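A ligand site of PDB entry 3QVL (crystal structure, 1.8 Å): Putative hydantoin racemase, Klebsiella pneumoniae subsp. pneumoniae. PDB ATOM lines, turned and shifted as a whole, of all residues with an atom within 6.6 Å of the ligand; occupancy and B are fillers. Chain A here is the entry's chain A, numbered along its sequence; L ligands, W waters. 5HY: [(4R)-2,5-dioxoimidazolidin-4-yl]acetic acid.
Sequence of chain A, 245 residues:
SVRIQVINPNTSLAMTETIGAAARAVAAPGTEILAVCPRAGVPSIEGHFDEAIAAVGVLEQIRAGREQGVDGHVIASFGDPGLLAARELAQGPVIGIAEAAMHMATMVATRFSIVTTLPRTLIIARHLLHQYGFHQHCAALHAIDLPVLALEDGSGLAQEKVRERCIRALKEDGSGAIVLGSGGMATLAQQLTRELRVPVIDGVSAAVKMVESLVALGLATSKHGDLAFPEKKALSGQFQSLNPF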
ATOM      1  N   ASN A   8     -16.842 -20.490  -9.963  1.00  0.00           N
ATOM      2  CA  ASN A   8     -15.432 -20.476  -9.625  1.00  0.00           C
ATOM      3  C   ASN A   8     -15.194 -21.552  -8.569  1.00  0.00           C
ATOM      4  O   ASN A   8     -15.724 -21.455  -7.465  1.00  0.00           O
ATOM      5  CB  ASN A   8     -15.015 -19.091  -9.097  1.00  0.00           C
ATOM      6  CG  ASN A   8     -13.555 -19.040  -8.662  1.00  0.00           C
ATOM      7  OD1 ASN A   8     -12.746 -19.898  -9.030  1.00  0.00           O
ATOM      8  ND2 ASN A   8     -13.207 -18.020  -7.889  1.00  0.00           N
ATOM      9  N   PRO A   9     -14.428 -22.605  -8.918  1.00  0.00           N
ATOM     10  CA  PRO A   9     -14.204 -23.733  -8.013  1.00  0.00           C
ATOM     11  C   PRO A   9     -13.346 -23.398  -6.800  1.00  0.00           C
ATOM     12  O   PRO A   9     -13.390 -24.141  -5.808  1.00  0.00           O
ATOM     13  CB  PRO A   9     -13.493 -24.761  -8.906  1.00  0.00           C
ATOM     14  CG  PRO A   9     -13.909 -24.392 -10.290  1.00  0.00           C
ATOM     15  CD  PRO A   9     -13.894 -22.893 -10.262  1.00  0.00           C
ATOM     16  N   ASN A  10     -12.580 -22.319  -6.861  1.00  0.00           N
ATOM     17  CA  ASN A  10     -11.857 -21.831  -5.677  1.00  0.00           C
ATOM     18  C   ASN A  10     -12.678 -20.780  -4.924  1.00  0.00           C
ATOM     19  O   ASN A  10     -13.658 -20.252  -5.454  1.00  0.00           O
ATOM     20  CB  ASN A  10     -10.451 -21.333  -6.026  1.00  0.00           C
ATOM     21  CG  ASN A  10     -10.455 -20.032  -6.809  1.00  0.00           C
ATOM     22  OD1 ASN A  10     -10.995 -19.017  -6.378  1.00  0.00           O
ATOM     23  ND2 ASN A  10      -9.807 -20.056  -7.973  1.00  0.00           N
ATOM     24  N   MET A  15     -11.095 -13.611  -7.691  1.00  0.00           N
ATOM     25  CA  MET A  15     -11.096 -14.389  -8.934  1.00  0.00           C
ATOM     26  C   MET A  15     -12.527 -14.606  -9.452  1.00  0.00           C
ATOM     27  O   MET A  15     -12.747 -14.611 -10.671  1.00  0.00           O
ATOM     28  CB  MET A  15     -10.357 -15.718  -8.737  1.00  0.00           C
ATOM     29  CG  MET A  15     -10.224 -16.579  -9.997  1.00  0.00           C
ATOM     30  SD  MET A  15      -8.589 -17.294 -10.295  1.00  0.00           S
ATOM     31  CE  MET A  15      -7.944 -17.479  -8.634  1.00  0.00           C
ATOM     32  N   ILE A  19     -13.800 -13.700 -13.184  1.00  0.00           N
ATOM     33  CA  ILE A  19     -14.543 -14.710 -13.938  1.00  0.00           C
ATOM     34  C   ILE A  19     -15.943 -14.208 -14.319  1.00  0.00           C
ATOM     35  O   ILE A  19     -16.367 -14.341 -15.478  1.00  0.00           O
ATOM     36  CB  ILE A  19     -14.618 -16.043 -13.157  1.00  0.00           C
ATOM     37  CG1 ILE A  19     -13.249 -16.735 -13.157  1.00  0.00           C
ATOM     38  CG2 ILE A  19     -15.689 -16.959 -13.732  1.00  0.00           C
ATOM     39  CD1 ILE A  19     -13.054 -17.757 -12.059  1.00  0.00           C
ATOM     40  N   PRO A  43      -8.620 -21.301  -1.505  1.00  0.00           N
ATOM     41  CA  PRO A  43      -8.541 -19.978  -2.152  1.00  0.00           C
ATOM     42  C   PRO A  43      -8.024 -20.009  -3.604  1.00  0.00           C
ATOM     43  O   PRO A  43      -8.424 -19.165  -4.409  1.00  0.00           O
ATOM     44  CB  PRO A  43      -7.562 -19.203  -1.268  1.00  0.00           C
ATOM     45  CG  PRO A  43      -7.669 -19.870   0.066  1.00  0.00           C
ATOM     46  CD  PRO A  43      -7.834 -21.325  -0.253  1.00  0.00           C
ATOM     47  N   SER A  44      -7.148 -20.963  -3.915  1.00  0.00           N
ATOM     48  CA  SER A  44      -6.667 -21.177  -5.274  1.00  0.00           C
ATOM     49  C   SER A  44      -6.321 -22.639  -5.495  1.00  0.00           C
ATOM     50  O   SER A  44      -5.966 -23.350  -4.548  1.00  0.00           O
ATOM     51  CB  SER A  44      -5.464 -20.284  -5.587  1.00  0.00           C
ATOM     52  OG  SER A  44      -4.339 -20.635  -4.815  1.00  0.00           O
ATOM     53  N   ILE A  45      -6.427 -23.092  -6.736  1.00  0.00           N
ATOM     54  CA  ILE A  45      -6.194 -24.487  -7.074  1.00  0.00           C
ATOM     55  C   ILE A  45      -4.832 -24.653  -7.738  1.00  0.00           C
ATOM     56  O   ILE A  45      -4.607 -24.204  -8.870  1.00  0.00           O
ATOM     57  CB  ILE A  45      -7.326 -25.050  -7.962  1.00  0.00           C
ATOM     58  CG1 ILE A  45      -8.682 -24.850  -7.271  1.00  0.00           C
ATOM     59  CG2 ILE A  45      -7.102 -26.532  -8.247  1.00  0.00           C
ATOM     60  CD1 ILE A  45      -9.846 -24.682  -8.229  1.00  0.00           C
ATOM     61  N   GLU A  46      -3.915 -25.289  -7.020  1.00  0.00           N
ATOM     62  CA  GLU A  46      -2.510 -25.392  -7.432  1.00  0.00           C
ATOM     63  C   GLU A  46      -1.977 -26.808  -7.246  1.00  0.00           C
ATOM     64  O   GLU A  46      -0.898 -27.016  -6.678  1.00  0.00           O
ATOM     65  CB  GLU A  46      -1.659 -24.403  -6.641  1.00  0.00           C
ATOM     66  CG  GLU A  46      -2.024 -22.944  -6.849  1.00  0.00           C
ATOM     67  CD  GLU A  46      -1.249 -21.993  -5.948  1.00  0.00           C
ATOM     68  OE1 GLU A  46      -1.133 -22.275  -4.736  1.00  0.00           O
ATOM     69  OE2 GLU A  46      -0.770 -20.964  -6.455  1.00  0.00           O
ATOM     70  N   ALA A  76     -15.262 -22.957 -13.699  1.00  0.00           N
ATOM     71  CA  ALA A  76     -14.336 -21.888 -14.064  1.00  0.00           C
ATOM     72  C   ALA A  76     -12.917 -21.963 -13.493  1.00  0.00           C
ATOM     73  O   ALA A  76     -12.359 -20.957 -13.055  1.00  0.00           O
ATOM     74  CB  ALA A  76     -14.970 -20.522 -13.785  1.00  0.00           C
ATOM     75  N   SER A  77     -12.354 -23.171 -13.515  1.00  0.00           N
ATOM     76  CA  SER A  77     -10.941 -23.407 -13.213  1.00  0.00           C
ATOM     77  C   SER A  77     -10.341 -24.265 -14.321  1.00  0.00           C
ATOM     78  O   SER A  77     -11.006 -25.174 -14.826  1.00  0.00           O
ATOM     79  CB  SER A  77     -10.784 -24.098 -11.862  1.00  0.00           C
ATOM     80  OG  SER A  77      -9.416 -24.289 -11.533  1.00  0.00           O
ATOM     81  N   PHE A  78      -9.096 -23.975 -14.700  1.00  0.00           N
ATOM     82  CA  PHE A  78      -8.460 -24.643 -15.851  1.00  0.00           C
ATOM     83  C   PHE A  78      -8.180 -26.148 -15.710  1.00  0.00           C
ATOM     84  O   PHE A  78      -7.745 -26.790 -16.664  1.00  0.00           O
ATOM     85  CB  PHE A  78      -7.199 -23.888 -16.266  1.00  0.00           C
ATOM     86  CG  PHE A  78      -6.781 -24.141 -17.695  1.00  0.00           C
ATOM     87  CD1 PHE A  78      -7.515 -23.623 -18.756  1.00  0.00           C
ATOM     88  CD2 PHE A  78      -5.654 -24.914 -17.972  1.00  0.00           C
ATOM     89  CE1 PHE A  78      -7.130 -23.858 -20.071  1.00  0.00           C
ATOM     90  CE2 PHE A  78      -5.268 -25.165 -19.284  1.00  0.00           C
ATOM     91  CZ  PHE A  78      -6.006 -24.629 -20.335  1.00  0.00           C
ATOM     92  N   GLY A  79      -8.430 -26.710 -14.533  1.00  0.00           N
ATOM     93  CA  GLY A  79      -8.348 -28.153 -14.353  1.00  0.00           C
ATOM     94  C   GLY A  79      -9.686 -28.849 -14.550  1.00  0.00           C
ATOM     95  O   GLY A  79      -9.757 -30.077 -14.491  1.00  0.00           O
ATOM     96  N   ILE A  97     -13.879 -24.780 -18.386  1.00  0.00           N
ATOM     97  CA  ILE A  97     -13.222 -23.701 -19.127  1.00  0.00           C
ATOM     98  C   ILE A  97     -12.004 -24.152 -19.925  1.00  0.00           C
ATOM     99  O   ILE A  97     -11.719 -23.600 -20.989  1.00  0.00           O
ATOM    100  CB  ILE A  97     -12.891 -22.456 -18.244  1.00  0.00           C
ATOM    101  CG1 ILE A  97     -11.903 -22.800 -17.118  1.00  0.00           C
ATOM    102  CG2 ILE A  97     -14.181 -21.844 -17.703  1.00  0.00           C
ATOM    103  CD1 ILE A  97     -11.102 -21.605 -16.628  1.00  0.00           C
ATOM    104  N   THR A 116      -0.259 -21.084 -18.664  1.00  0.00           N
ATOM    105  CA  THR A 116      -0.849 -21.165 -17.327  1.00  0.00           C
ATOM    106  C   THR A 116       0.038 -20.460 -16.296  1.00  0.00           C
ATOM    107  O   THR A 116       1.017 -19.807 -16.659  1.00  0.00           O
ATOM    108  CB  THR A 116      -1.181 -22.635 -16.930  1.00  0.00           C
ATOM    109  OG1 THR A 116      -2.020 -22.641 -15.765  1.00  0.00           O
ATOM    110  CG2 THR A 116       0.086 -23.449 -16.677  1.00  0.00           C
ATOM    111  N   THR A 117      -0.307 -20.577 -15.012  1.00  0.00           N
ATOM    112  CA  THR A 117       0.366 -19.791 -13.963  1.00  0.00           C
ATOM    113  C   THR A 117       1.499 -20.556 -13.265  1.00  0.00           C
ATOM    114  O   THR A 117       2.659 -20.143 -13.343  1.00  0.00           O
ATOM    115  CB  THR A 117      -0.645 -19.214 -12.945  1.00  0.00           C
ATOM    116  OG1 THR A 117      -1.893 -18.940 -13.599  1.00  0.00           O
ATOM    117  CG2 THR A 117      -0.113 -17.939 -12.325  1.00  0.00           C
ATOM    118  N   LEU A 118       1.164 -21.638 -12.562  1.00  0.00           N
ATOM    119  CA  LEU A 118       2.150 -22.427 -11.817  1.00  0.00           C
ATOM    120  C   LEU A 118       2.638 -23.664 -12.579  1.00  0.00           C
ATOM    121  O   LEU A 118       1.822 -24.378 -13.181  1.00  0.00           O
ATOM    122  CB  LEU A 118       1.587 -22.883 -10.459  1.00  0.00           C
ATOM    123  CG  LEU A 118       1.938 -22.173  -9.144  1.00  0.00           C
ATOM    124  CD1 LEU A 118       1.536 -23.057  -7.989  1.00  0.00           C
ATOM    125  CD2 LEU A 118       3.418 -21.813  -9.026  1.00  0.00           C
ATOM    126  N   THR A 121       1.045 -27.244 -12.160  1.00  0.00           N
ATOM    127  CA  THR A 121      -0.287 -27.443 -12.736  1.00  0.00           C
ATOM    128  C   THR A 121      -0.222 -27.854 -14.211  1.00  0.00           C
ATOM    129  O   THR A 121      -1.240 -28.200 -14.803  1.00  0.00           O
ATOM    130  CB  THR A 121      -1.184 -26.186 -12.590  1.00  0.00           C
ATOM    131  OG1 THR A 121      -0.686 -25.129 -13.418  1.00  0.00           O
ATOM    132  CG2 THR A 121      -1.254 -25.720 -11.144  1.00  0.00           C
ATOM    133  N   VAL A 148      -1.051 -18.764  -8.407  1.00  0.00           N
ATOM    134  CA  VAL A 148      -2.308 -18.474  -9.109  1.00  0.00           C
ATOM    135  C   VAL A 148      -2.878 -17.102  -8.743  1.00  0.00           C
ATOM    136  O   VAL A 148      -3.317 -16.354  -9.619  1.00  0.00           O
ATOM    137  CB  VAL A 148      -3.346 -19.612  -8.859  1.00  0.00           C
ATOM    138  CG1 VAL A 148      -4.751 -19.163  -9.243  1.00  0.00           C
ATOM    139  CG2 VAL A 148      -2.956 -20.859  -9.629  1.00  0.00           C
ATOM    140  N   LEU A 149      -2.855 -16.773  -7.456  1.00  0.00           N
ATOM    141  CA  LEU A 149      -3.437 -15.529  -6.952  1.00  0.00           C
ATOM    142  C   LEU A 149      -2.626 -14.265  -7.273  1.00  0.00           C
ATOM    143  O   LEU A 149      -3.081 -13.157  -6.987  1.00  0.00           O
ATOM    144  CB  LEU A 149      -3.733 -15.629  -5.453  1.00  0.00           C
ATOM    145  CG  LEU A 149      -4.805 -16.648  -5.048  1.00  0.00           C
ATOM    146  CD1 LEU A 149      -4.859 -16.805  -3.541  1.00  0.00           C
ATOM    147  CD2 LEU A 149      -6.174 -16.260  -5.592  1.00  0.00           C
ATOM    148  N   LEU A 151      -2.288 -13.143 -10.113  1.00  0.00           N
ATOM    149  CA  LEU A 151      -3.133 -12.485 -11.101  1.00  0.00           C
ATOM    150  C   LEU A 151      -4.106 -11.489 -10.467  1.00  0.00           C
ATOM    151  O   LEU A 151      -4.656 -10.619 -11.150  1.00  0.00           O
ATOM    152  CB  LEU A 151      -3.911 -13.519 -11.927  1.00  0.00           C
ATOM    153  CG  LEU A 151      -3.117 -14.335 -12.948  1.00  0.00           C
ATOM    154  CD1 LEU A 151      -3.812 -15.661 -13.237  1.00  0.00           C
ATOM    155  CD2 LEU A 151      -2.901 -13.553 -14.247  1.00  0.00           C
ATOM    156  N   GLY A 181      -4.517 -20.355 -19.578  1.00  0.00           N
ATOM    157  CA  GLY A 181      -4.638 -21.480 -18.663  1.00  0.00           C
ATOM    158  C   GLY A 181      -5.050 -21.128 -17.245  1.00  0.00           C
ATOM    159  O   GLY A 181      -4.624 -21.797 -16.300  1.00  0.00           O
ATOM    160  N   SER A 182      -5.875 -20.098 -17.099  1.00  0.00           N
ATOM    161  CA  SER A 182      -6.333 -19.649 -15.791  1.00  0.00           C
ATOM    162  C   SER A 182      -7.651 -18.881 -15.875  1.00  0.00           C
ATOM    163  O   SER A 182      -7.872 -18.108 -16.810  1.00  0.00           O
ATOM    164  CB  SER A 182      -5.280 -18.757 -15.129  1.00  0.00           C
ATOM    165  OG  SER A 182      -5.743 -18.264 -13.879  1.00  0.00           O
ATOM    166  N   GLY A 183      -8.519 -19.109 -14.897  1.00  0.00           N
ATOM    167  CA  GLY A 183      -9.725 -18.307 -14.730  1.00  0.00           C
ATOM    168  C   GLY A 183      -9.391 -16.862 -14.391  1.00  0.00           C
ATOM    169  O   GLY A 183     -10.167 -15.954 -14.687  1.00  0.00           O
ATOM    170  N   GLY A 184      -8.224 -16.668 -13.774  1.00  0.00           N
ATOM    171  CA  GLY A 184      -7.734 -15.336 -13.427  1.00  0.00           C
ATOM    172  C   GLY A 184      -7.212 -14.533 -14.616  1.00  0.00           C
ATOM    173  O   GLY A 184      -6.999 -13.324 -14.498  1.00  0.00           O
ATOM    174  N   MET A 185      -7.007 -15.210 -15.747  1.00  0.00           N
ATOM    175  CA  MET A 185      -6.540 -14.564 -16.975  1.00  0.00           C
ATOM    176  C   MET A 185      -7.704 -14.179 -17.893  1.00  0.00           C
ATOM    177  O   MET A 185      -7.491 -13.636 -18.973  1.00  0.00           O
ATOM    178  CB  MET A 185      -5.586 -15.491 -17.731  1.00  0.00           C
ATOM    179  CG  MET A 185      -4.252 -15.742 -17.059  1.00  0.00           C
ATOM    180  SD  MET A 185      -3.273 -16.940 -17.975  1.00  0.00           S
ATOM    181  CE  MET A 185      -2.064 -17.410 -16.729  1.00  0.00           C
HETATM  182  C   5HY L   1      -7.621 -21.841 -12.320  1.00  0.00           C
HETATM  183  N   5HY L   1      -6.405 -22.764 -10.595  1.00  0.00           N
HETATM  184  O   5HY L   1      -8.082 -21.555 -13.427  1.00  0.00           O
HETATM  185  CA  5HY L   1      -6.558 -22.895 -12.053  1.00  0.00           C
HETATM  186  CB  5HY L   1      -5.240 -22.627 -12.808  1.00  0.00           C
HETATM  187  CG  5HY L   1      -4.680 -21.199 -12.704  1.00  0.00           C
HETATM  188  OAB 5HY L   1      -7.409 -21.524  -8.993  1.00  0.00           O
HETATM  189  NAF 5HY L   1      -7.989 -21.287 -11.164  1.00  0.00           N
HETATM  190  CAI 5HY L   1      -7.284 -21.836 -10.179  1.00  0.00           C
HETATM  191  OD1 5HY L   1      -3.514 -21.040 -13.124  1.00  0.00           O
HETATM  192  OD2 5HY L   1      -5.405 -20.301 -12.225  1.00  0.00           O
HETATM  193  O   HOH W   1      -1.433 -22.632 -12.720  1.00  0.00           O
HETATM  194  O   HOH W   2     -10.648 -20.316 -10.876  1.00  0.00           O
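Water W1 lies within hydrogen-bond range of an oxygen (OD1) of the ligand (2.7 Å), the side-chain hydroxyl of Thr 121 (2.7 Å), the backbone NH of Leu 118 (2.8 Å), the side-chain hydroxyl of Thr 116 (3.1 Å) and the backbone NH of Thr 117 (3.3 Å).
The side-chain amide oxygen (OD1) of Asn 10 sits at hydrogen-bond distance from the side-chain amide nitrogen (ND2) of Asn 8 (2.9 Å).
OG1 of Thr 116 lies within hydrogen-bond range of O of Gly 181, 2.8 Å away.
The side-chain amide oxygen (OD1) of Asn 10 lies close to the backbone carbonyl oxygen (O) of Pro 43 (3.2 Å).
The side-chain carboxylate (OE2) of Glu 46 sits at hydrogen-bond distance from the backbone NH (N) of Val 148 (3.0 Å).
The side-chain hydroxyl of Ser 182 sits at hydrogen-bond distance from the backbone NH of Gly 184 (3.0 Å).
An oxygen (OD1) of the ligand sits close to the backbone carbonyl oxygen (O) of Gly 181 (3.4 Å).
CA of Ser 44 touches OAB of the ligand, 3.8 Å away.
Val 148 touches the ligand (CG1 to OD2, 3.3 Å).
Hydrophobic or aromatic side chains that line the ligand: Ile 45, Phe 78 and Val 148.
Of the 26 residues printed, 11 come within 4 Å of the ligand.
An oxygen (OAB) of the ligand sits at hydrogen-bond distance from the backbone NH (N) of Ile 45 (2.9 Å).
A nitrogen (NAF) of the ligand lies close to the side-chain hydroxyl (OG) of Ser 77, 3.3 Å away.
The backbone carbonyl oxygen of Ile 45 lies within hydrogen-bond range of a nitrogen (N) of the ligand.
The backbone NH of Phe 78 is in hydrogen-bond range of an oxygen (O) of the ligand (2.9 Å).
An oxygen (OD1) of the ligand is in hydrogen-bond range of the side-chain hydroxyl (OG1) of Thr 116 (3.4 Å).
The side-chain amide nitrogen (ND2) of Asn 10 sits at hydrogen-bond distance from an oxygen (OAB) of the ligand (3.0 Å).
An oxygen (OD1) of the ligand sits at hydrogen-bond distance from the side-chain hydroxyl (OG1) of Thr 117, at 2.7 Å.
The backbone NH (N) of Gly 183 lies within hydrogen-bond range of an oxygen (O) of the ligand (2.9 Å).
OD2 of the ligand sits at hydrogen-bond distance from OG of Ser 182.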
